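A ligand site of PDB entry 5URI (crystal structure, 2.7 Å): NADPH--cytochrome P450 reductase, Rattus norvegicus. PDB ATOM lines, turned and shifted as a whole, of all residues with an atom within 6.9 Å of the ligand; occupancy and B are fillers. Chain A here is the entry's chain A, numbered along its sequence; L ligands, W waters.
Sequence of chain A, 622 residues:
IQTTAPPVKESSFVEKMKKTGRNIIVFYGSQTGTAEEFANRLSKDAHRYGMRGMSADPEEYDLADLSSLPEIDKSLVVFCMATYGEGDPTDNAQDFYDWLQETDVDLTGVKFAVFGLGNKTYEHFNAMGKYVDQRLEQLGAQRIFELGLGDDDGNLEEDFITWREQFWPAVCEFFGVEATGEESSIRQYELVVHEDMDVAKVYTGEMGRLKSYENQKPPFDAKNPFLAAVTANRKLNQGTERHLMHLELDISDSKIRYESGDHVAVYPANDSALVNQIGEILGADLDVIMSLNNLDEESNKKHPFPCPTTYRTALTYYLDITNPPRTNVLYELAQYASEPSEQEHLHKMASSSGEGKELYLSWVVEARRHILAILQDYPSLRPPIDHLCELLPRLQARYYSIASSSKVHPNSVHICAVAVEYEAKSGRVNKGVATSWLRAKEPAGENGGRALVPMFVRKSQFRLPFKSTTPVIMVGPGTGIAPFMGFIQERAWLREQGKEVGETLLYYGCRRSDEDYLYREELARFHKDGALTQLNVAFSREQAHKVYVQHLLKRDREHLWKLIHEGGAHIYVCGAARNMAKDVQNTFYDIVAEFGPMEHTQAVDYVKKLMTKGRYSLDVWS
OG of Ser 540 sits at hydrogen-bond distance from O3 of the ligand, 2.6 Å away.
The side-chain hydroxyl of Tyr 548 is in hydrogen-bond range of an oxygen (O1) of the ligand.
NH2 of Arg 541 lies within salt-bridge range of O2 of the ligand.
A nitrogen (N4) of the ligand lies within hydrogen-bond range of the side-chain amide nitrogen (NE2) of Gln 550 (2.9 Å).
OD2 of Asp 583 sits at hydrogen-bond distance from N3 of the ligand.
The backbone carbonyl oxygen (O) of Cys 510 lies close to an oxygen (O6) of the ligand (3.2 Å).
An oxygen (O3) of the ligand is in salt-bridge range of the side-chain amino group (NZ) of Lys 546.
The backbone NH (N) of Ser 540 sits at hydrogen-bond distance from the backbone carbonyl oxygen (O) of Cys 510 (2.8 Å).
The backbone carbonyl oxygen (O) of Arg 511 lies within hydrogen-bond range of the backbone NH (N) of Arg 541.
The side-chain amide nitrogen of Gln 550 sits close to the side-chain carboxylate of Asp 583 (3.5 Å).
The backbone carbonyl oxygen of Ala 538 is in hydrogen-bond range of the backbone NH of Cys 510, 3.1 Å away.
The side-chain sulfur (SG) of Cys 510 is in hydrogen-bond range of the backbone carbonyl oxygen (O) of Arg 512, at 3.7 Å.
N of Gly 478 lies within hydrogen-bond range of O of Gly 509, at 2.8 Å.
The guanidinium group (NE) of Arg 511 is in salt-bridge range of the side-chain carboxylate (OD2) of Asp 516.
Merely in contact with the ligand: Pro 477, Gly 478, Arg 511 and Met 580.
Hydrophobic or aromatic side chains that line the ligand: Pro 477, Tyr 548 and Met 580.
Within 4 Å of the ligand: Pro 477, Gly 478, Cys 510, Arg 511, Ser 540, Arg 541, Lys 546, Tyr 548, Gln 550, Met 580 and Asp 583.
The nearest printed residue that does not touch the ligand is Val 549 (4.03 Å).
Water W3 lies within hydrogen-bond range of an oxygen (O6) of the ligand, the backbone carbonyl oxygen (O) of Ala 538 and the backbone NH (N) of Cys 510.
Water W1 bridges N5 of the ligand (2.8 Å) and N of Val 549 (2.8 Å).
Water W2 lies within hydrogen-bond range of OD2 of Asp 516, NH1 of Arg 242 and N of Arg 511.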
ATOM      1  N   ARG A 242     -23.442  44.254  -1.022  1.00  0.00           N
ATOM      2  CA  ARG A 242     -22.615  44.201  -2.217  1.00  0.00           C
ATOM      3  C   ARG A 242     -23.417  44.782  -3.374  1.00  0.00           C
ATOM      4  O   ARG A 242     -24.562  45.186  -3.202  1.00  0.00           O
ATOM      5  CB  ARG A 242     -22.273  42.734  -2.531  1.00  0.00           C
ATOM      6  CG  ARG A 242     -22.074  41.863  -1.313  1.00  0.00           C
ATOM      7  CD  ARG A 242     -22.809  40.551  -1.454  1.00  0.00           C
ATOM      8  NE  ARG A 242     -22.130  39.635  -2.356  1.00  0.00           N
ATOM      9  CZ  ARG A 242     -22.648  38.489  -2.789  1.00  0.00           C
ATOM     10  NH1 ARG A 242     -23.863  38.110  -2.399  1.00  0.00           N
ATOM     11  NH2 ARG A 242     -21.934  37.700  -3.599  1.00  0.00           N
ATOM     12  N   PRO A 477     -25.437  28.469  -7.518  1.00  0.00           N
ATOM     13  CA  PRO A 477     -25.643  29.435  -6.423  1.00  0.00           C
ATOM     14  C   PRO A 477     -25.072  30.814  -6.760  1.00  0.00           C
ATOM     15  O   PRO A 477     -24.315  30.967  -7.728  1.00  0.00           O
ATOM     16  CB  PRO A 477     -24.914  28.768  -5.248  1.00  0.00           C
ATOM     17  CG  PRO A 477     -23.767  28.075  -5.927  1.00  0.00           C
ATOM     18  CD  PRO A 477     -24.425  27.454  -7.147  1.00  0.00           C
ATOM     19  N   GLY A 478     -25.454  31.814  -5.963  1.00  0.00           N
ATOM     20  CA  GLY A 478     -24.979  33.164  -6.172  1.00  0.00           C
ATOM     21  C   GLY A 478     -25.065  33.628  -7.613  1.00  0.00           C
ATOM     22  O   GLY A 478     -26.102  33.491  -8.231  1.00  0.00           O
ATOM     23  N   THR A 479     -23.976  34.168  -8.142  1.00  0.00           N
ATOM     24  CA  THR A 479     -23.972  34.635  -9.525  1.00  0.00           C
ATOM     25  C   THR A 479     -23.940  33.494 -10.530  1.00  0.00           C
ATOM     26  O   THR A 479     -24.023  33.734 -11.727  1.00  0.00           O
ATOM     27  CB  THR A 479     -22.783  35.589  -9.817  1.00  0.00           C
ATOM     28  OG1 THR A 479     -21.556  34.943  -9.443  1.00  0.00           O
ATOM     29  CG2 THR A 479     -22.927  36.876  -9.031  1.00  0.00           C
ATOM     30  N   GLY A 480     -23.789  32.265 -10.052  1.00  0.00           N
ATOM     31  CA  GLY A 480     -23.777  31.124 -10.951  1.00  0.00           C
ATOM     32  C   GLY A 480     -25.073  31.044 -11.761  1.00  0.00           C
ATOM     33  O   GLY A 480     -25.115  30.424 -12.825  1.00  0.00           O
ATOM     34  N   GLY A 509     -29.094  29.583  -5.055  1.00  0.00           N
ATOM     35  CA  GLY A 509     -28.819  29.953  -3.687  1.00  0.00           C
ATOM     36  C   GLY A 509     -28.327  31.374  -3.482  1.00  0.00           C
ATOM     37  O   GLY A 509     -27.682  31.967  -4.356  1.00  0.00           O
ATOM     38  N   CYS A 510     -28.660  31.943  -2.331  1.00  0.00           N
ATOM     39  CA  CYS A 510     -28.226  33.287  -1.994  1.00  0.00           C
ATOM     40  C   CYS A 510     -28.256  33.386  -0.480  1.00  0.00           C
ATOM     41  O   CYS A 510     -28.625  32.428   0.195  1.00  0.00           O
ATOM     42  CB  CYS A 510     -29.143  34.331  -2.633  1.00  0.00           C
ATOM     43  SG  CYS A 510     -30.850  34.212  -2.105  1.00  0.00           S
ATOM     44  N   ARG A 511     -27.863  34.526   0.063  1.00  0.00           N
ATOM     45  CA  ARG A 511     -27.856  34.707   1.505  1.00  0.00           C
ATOM     46  C   ARG A 511     -29.273  34.866   2.079  1.00  0.00           C
ATOM     47  O   ARG A 511     -29.681  34.132   2.979  1.00  0.00           O
ATOM     48  CB  ARG A 511     -26.978  35.904   1.866  1.00  0.00           C
ATOM     49  CG  ARG A 511     -25.575  35.854   1.261  1.00  0.00           C
ATOM     50  CD  ARG A 511     -24.789  37.102   1.616  1.00  0.00           C
ATOM     51  NE  ARG A 511     -23.401  37.050   1.154  1.00  0.00           N
ATOM     52  CZ  ARG A 511     -22.523  38.046   1.301  1.00  0.00           C
ATOM     53  NH1 ARG A 511     -22.880  39.178   1.909  1.00  0.00           N
ATOM     54  NH2 ARG A 511     -21.291  37.907   0.850  1.00  0.00           N
ATOM     55  N   ARG A 512     -30.021  35.833   1.557  1.00  0.00           N
ATOM     56  CA  ARG A 512     -31.385  36.085   2.025  1.00  0.00           C
ATOM     57  C   ARG A 512     -32.232  36.556   0.846  1.00  0.00           C
ATOM     58  O   ARG A 512     -31.727  37.215  -0.065  1.00  0.00           O
ATOM     59  CB  ARG A 512     -31.390  37.182   3.099  1.00  0.00           C
ATOM     60  CG  ARG A 512     -30.505  36.897   4.286  1.00  0.00           C
ATOM     61  CD  ARG A 512     -30.763  37.924   5.375  1.00  0.00           C
ATOM     62  NE  ARG A 512     -29.911  37.716   6.535  1.00  0.00           N
ATOM     63  CZ  ARG A 512     -28.582  37.837   6.515  1.00  0.00           C
ATOM     64  NH1 ARG A 512     -27.956  38.156   5.384  1.00  0.00           N
ATOM     65  NH2 ARG A 512     -27.879  37.625   7.623  1.00  0.00           N
ATOM     66  N   ASP A 516     -29.897  39.493  -1.617  1.00  0.00           N
ATOM     67  CA  ASP A 516     -29.381  39.195  -2.939  1.00  0.00           C
ATOM     68  C   ASP A 516     -30.089  38.096  -3.754  1.00  0.00           C
ATOM     69  O   ASP A 516     -29.424  37.300  -4.416  1.00  0.00           O
ATOM     70  CB  ASP A 516     -27.890  38.855  -2.837  1.00  0.00           C
ATOM     71  CG  ASP A 516     -27.588  37.920  -1.669  1.00  0.00           C
ATOM     72  OD1 ASP A 516     -28.514  37.195  -1.233  1.00  0.00           O
ATOM     73  OD2 ASP A 516     -26.428  37.920  -1.207  1.00  0.00           O
ATOM     74  N   ALA A 538     -32.015  27.934  -1.980  1.00  0.00           N
ATOM     75  CA  ALA A 538     -31.407  27.767  -0.662  1.00  0.00           C
ATOM     76  C   ALA A 538     -30.890  29.092  -0.127  1.00  0.00           C
ATOM     77  O   ALA A 538     -29.913  29.633  -0.653  1.00  0.00           O
ATOM     78  CB  ALA A 538     -30.263  26.782  -0.750  1.00  0.00           C
ATOM     79  N   PHE A 539     -31.544  29.610   0.906  1.00  0.00           N
ATOM     80  CA  PHE A 539     -31.129  30.877   1.535  1.00  0.00           C
ATOM     81  C   PHE A 539     -30.158  30.556   2.673  1.00  0.00           C
ATOM     82  O   PHE A 539     -30.564  30.214   3.790  1.00  0.00           O
ATOM     83  CB  PHE A 539     -32.343  31.623   2.093  1.00  0.00           C
ATOM     84  CG  PHE A 539     -33.352  31.967   1.049  1.00  0.00           C
ATOM     85  CD1 PHE A 539     -33.031  32.830   0.006  1.00  0.00           C
ATOM     86  CD2 PHE A 539     -34.623  31.400   1.084  1.00  0.00           C
ATOM     87  CE1 PHE A 539     -33.956  33.127  -0.988  1.00  0.00           C
ATOM     88  CE2 PHE A 539     -35.552  31.694   0.098  1.00  0.00           C
ATOM     89  CZ  PHE A 539     -35.214  32.560  -0.946  1.00  0.00           C
ATOM     90  N   SER A 540     -28.870  30.668   2.386  1.00  0.00           N
ATOM     91  CA  SER A 540     -27.849  30.336   3.359  1.00  0.00           C
ATOM     92  C   SER A 540     -27.836  31.108   4.677  1.00  0.00           C
ATOM     93  O   SER A 540     -27.282  30.627   5.649  1.00  0.00           O
ATOM     94  CB  SER A 540     -26.460  30.425   2.722  1.00  0.00           C
ATOM     95  OG  SER A 540     -26.179  31.752   2.315  1.00  0.00           O
ATOM     96  N   ARG A 541     -28.455  32.294   4.730  1.00  0.00           N
ATOM     97  CA  ARG A 541     -28.407  33.044   5.976  1.00  0.00           C
ATOM     98  C   ARG A 541     -29.702  33.425   6.658  1.00  0.00           C
ATOM     99  O   ARG A 541     -29.707  34.316   7.505  1.00  0.00           O
ATOM    100  CB  ARG A 541     -27.568  34.311   5.795  1.00  0.00           C
ATOM    101  CG  ARG A 541     -26.190  34.022   5.219  1.00  0.00           C
ATOM    102  CD  ARG A 541     -25.296  35.231   5.116  1.00  0.00           C
ATOM    103  NE  ARG A 541     -24.068  34.878   4.410  1.00  0.00           N
ATOM    104  CZ  ARG A 541     -23.023  35.686   4.279  1.00  0.00           C
ATOM    105  NH1 ARG A 541     -23.044  36.905   4.815  1.00  0.00           N
ATOM    106  NH2 ARG A 541     -21.953  35.277   3.605  1.00  0.00           N
ATOM    107  N   LYS A 546     -26.279  26.924   7.723  1.00  0.00           N
ATOM    108  CA  LYS A 546     -26.232  27.241   6.314  1.00  0.00           C
ATOM    109  C   LYS A 546     -27.120  26.260   5.563  1.00  0.00           C
ATOM    110  O   LYS A 546     -27.144  25.061   5.869  1.00  0.00           O
ATOM    111  CB  LYS A 546     -24.800  27.107   5.790  1.00  0.00           C
ATOM    112  CG  LYS A 546     -23.781  27.954   6.494  1.00  0.00           C
ATOM    113  CD  LYS A 546     -24.038  29.415   6.269  1.00  0.00           C
ATOM    114  CE  LYS A 546     -22.900  30.265   6.813  1.00  0.00           C
ATOM    115  NZ  LYS A 546     -23.148  31.731   6.571  1.00  0.00           N
ATOM    116  N   VAL A 547     -27.871  26.772   4.606  1.00  0.00           N
ATOM    117  CA  VAL A 547     -28.704  25.905   3.779  1.00  0.00           C
ATOM    118  C   VAL A 547     -28.110  26.169   2.394  1.00  0.00           C
ATOM    119  O   VAL A 547     -28.257  27.253   1.826  1.00  0.00           O
ATOM    120  CB  VAL A 547     -30.196  26.295   3.855  1.00  0.00           C
ATOM    121  CG1 VAL A 547     -31.019  25.380   2.960  1.00  0.00           C
ATOM    122  CG2 VAL A 547     -30.682  26.180   5.283  1.00  0.00           C
ATOM    123  N   TYR A 548     -27.391  25.181   1.872  1.00  0.00           N
ATOM    124  CA  TYR A 548     -26.751  25.337   0.581  1.00  0.00           C
ATOM    125  C   TYR A 548     -27.485  24.562  -0.505  1.00  0.00           C
ATOM    126  O   TYR A 548     -28.268  23.654  -0.206  1.00  0.00           O
ATOM    127  CB  TYR A 548     -25.298  24.880   0.662  1.00  0.00           C
ATOM    128  CG  TYR A 548     -24.426  25.777   1.506  1.00  0.00           C
ATOM    129  CD1 TYR A 548     -24.665  27.157   1.578  1.00  0.00           C
ATOM    130  CD2 TYR A 548     -23.303  25.271   2.174  1.00  0.00           C
ATOM    131  CE1 TYR A 548     -23.817  27.999   2.277  1.00  0.00           C
ATOM    132  CE2 TYR A 548     -22.448  26.107   2.875  1.00  0.00           C
ATOM    133  CZ  TYR A 548     -22.706  27.476   2.921  1.00  0.00           C
ATOM    134  OH  TYR A 548     -21.855  28.318   3.599  1.00  0.00           O
ATOM    135  N   VAL A 549     -27.227  24.913  -1.752  1.00  0.00           N
ATOM    136  CA  VAL A 549     -27.909  24.224  -2.831  1.00  0.00           C
ATOM    137  C   VAL A 549     -27.796  22.687  -2.748  1.00  0.00           C
ATOM    138  O   VAL A 549     -28.801  21.988  -2.935  1.00  0.00           O
ATOM    139  CB  VAL A 549     -27.429  24.714  -4.237  1.00  0.00           C
ATOM    140  CG1 VAL A 549     -27.941  26.124  -4.490  1.00  0.00           C
ATOM    141  CG2 VAL A 549     -25.892  24.673  -4.331  1.00  0.00           C
ATOM    142  N   GLN A 550     -26.605  22.162  -2.459  1.00  0.00           N
ATOM    143  CA  GLN A 550     -26.430  20.716  -2.386  1.00  0.00           C
ATOM    144  C   GLN A 550     -27.308  20.078  -1.329  1.00  0.00           C
ATOM    145  O   GLN A 550     -27.612  18.890  -1.413  1.00  0.00           O
ATOM    146  CB  GLN A 550     -24.972  20.333  -2.104  1.00  0.00           C
ATOM    147  CG  GLN A 550     -24.396  20.975  -0.861  1.00  0.00           C
ATOM    148  CD  GLN A 550     -23.709  22.279  -1.164  1.00  0.00           C
ATOM    149  OE1 GLN A 550     -24.200  23.094  -1.953  1.00  0.00           O
ATOM    150  NE2 GLN A 550     -22.559  22.487  -0.549  1.00  0.00           N
ATOM    151  N   ASN A 579     -14.863  24.742  -4.361  1.00  0.00           N
ATOM    152  CA  ASN A 579     -15.260  24.277  -3.045  1.00  0.00           C
ATOM    153  C   ASN A 579     -16.730  23.889  -3.192  1.00  0.00           C
ATOM    154  O   ASN A 579     -17.144  22.796  -2.814  1.00  0.00           O
ATOM    155  CB  ASN A 579     -15.085  25.391  -2.015  1.00  0.00           C
ATOM    156  CG  ASN A 579     -15.180  24.910  -0.589  1.00  0.00           C
ATOM    157  OD1 ASN A 579     -14.799  25.623   0.348  1.00  0.00           O
ATOM    158  ND2 ASN A 579     -15.709  23.705  -0.396  1.00  0.00           N
ATOM    159  N   MET A 580     -17.508  24.796  -3.782  1.00  0.00           N
ATOM    160  CA  MET A 580     -18.937  24.592  -4.024  1.00  0.00           C
ATOM    161  C   MET A 580     -19.149  23.448  -5.012  1.00  0.00           C
ATOM    162  O   MET A 580     -19.880  22.511  -4.754  1.00  0.00           O
ATOM    163  CB  MET A 580     -19.560  25.886  -4.566  1.00  0.00           C
ATOM    164  CG  MET A 580     -21.064  25.856  -4.861  1.00  0.00           C
ATOM    165  SD  MET A 580     -21.546  25.016  -6.410  1.00  0.00           S
ATOM    166  CE  MET A 580     -20.640  25.941  -7.629  1.00  0.00           C
ATOM    167  N   ALA A 581     -18.475  23.524  -6.150  1.00  0.00           N
ATOM    168  CA  ALA A 581     -18.594  22.460  -7.148  1.00  0.00           C
ATOM    169  C   ALA A 581     -18.237  21.105  -6.549  1.00  0.00           C
ATOM    170  O   ALA A 581     -18.889  20.109  -6.851  1.00  0.00           O
ATOM    171  CB  ALA A 581     -17.711  22.768  -8.352  1.00  0.00           C
ATOM    172  N   ASP A 583     -18.498  20.050  -3.366  1.00  0.00           N
ATOM    173  CA  ASP A 583     -19.603  19.648  -2.499  1.00  0.00           C
ATOM    174  C   ASP A 583     -20.749  19.068  -3.323  1.00  0.00           C
ATOM    175  O   ASP A 583     -21.260  17.987  -3.035  1.00  0.00           O
ATOM    176  CB  ASP A 583     -20.122  20.828  -1.690  1.00  0.00           C
ATOM    177  CG  ASP A 583     -19.103  21.364  -0.723  1.00  0.00           C
ATOM    178  OD1 ASP A 583     -18.322  20.551  -0.184  1.00  0.00           O
ATOM    179  OD2 ASP A 583     -19.081  22.582  -0.480  1.00  0.00           O
ATOM    180  N   VAL A 584     -21.144  19.803  -4.356  1.00  0.00           N
ATOM    181  CA  VAL A 584     -22.227  19.351  -5.224  1.00  0.00           C
ATOM    182  C   VAL A 584     -21.862  18.016  -5.869  1.00  0.00           C
ATOM    183  O   VAL A 584     -22.686  17.109  -5.996  1.00  0.00           O
ATOM    184  CB  VAL A 584     -22.517  20.411  -6.335  1.00  0.00           C
ATOM    185  CG1 VAL A 584     -23.482  19.846  -7.365  1.00  0.00           C
ATOM    186  CG2 VAL A 584     -23.098  21.681  -5.703  1.00  0.00           C
HETATM  187  P1  LIG L   1     -22.807  31.902   2.407  1.00  0.00           P
HETATM  188  O1  LIG L   1     -21.790  30.894   2.782  1.00  0.00           O
HETATM  189  O2  LIG L   1     -22.257  33.135   1.804  1.00  0.00           O
HETATM  190  O3  LIG L   1     -23.831  32.142   3.446  1.00  0.00           O
HETATM  191  C1  LIG L   1     -23.646  32.969  -3.224  1.00  0.00           C
HETATM  192  O4  LIG L   1     -22.391  33.499  -2.780  1.00  0.00           O
HETATM  193  C2  LIG L   1     -24.096  31.795  -2.344  1.00  0.00           C
HETATM  194  O5  LIG L   1     -23.113  30.743  -2.301  1.00  0.00           O
HETATM  195  C3  LIG L   1     -24.304  32.231  -0.906  1.00  0.00           C
HETATM  196  O6  LIG L   1     -25.596  31.784  -0.460  1.00  0.00           O
HETATM  197  C4  LIG L   1     -23.246  31.441  -0.163  1.00  0.00           C
HETATM  198  O7  LIG L   1     -23.635  31.212   1.208  1.00  0.00           O
HETATM  199  C5  LIG L   1     -23.300  30.172  -0.995  1.00  0.00           C
HETATM  200  N1  LIG L   1     -22.259  29.186  -0.636  1.00  0.00           N
HETATM  201  C6  LIG L   1     -21.141  29.432   0.045  1.00  0.00           C
HETATM  202  N2  LIG L   1     -20.463  28.291   0.129  1.00  0.00           N
HETATM  203  C7  LIG L   1     -21.165  27.340  -0.486  1.00  0.00           C
HETATM  204  C8  LIG L   1     -20.945  26.032  -0.613  1.00  0.00           C
HETATM  205  N3  LIG L   1     -19.787  25.581  -0.143  1.00  0.00           N
HETATM  206  N4  LIG L   1     -21.816  25.224  -1.232  1.00  0.00           N
HETATM  207  C9  LIG L   1     -22.978  25.789  -1.773  1.00  0.00           C
HETATM  208  N5  LIG L   1     -23.181  27.165  -1.615  1.00  0.00           N
HETATM  209  C10 LIG L   1     -22.266  27.905  -0.973  1.00  0.00           C
HETATM  210  O   HOH W   1     -25.860  27.300  -2.479  1.00  0.00           O
HETATM  211  O   HOH W   2     -25.849  35.377  -2.601  1.00  0.00           O
HETATM  212  O   HOH W   3     -27.015  29.402  -0.744  1.00  0.00           O
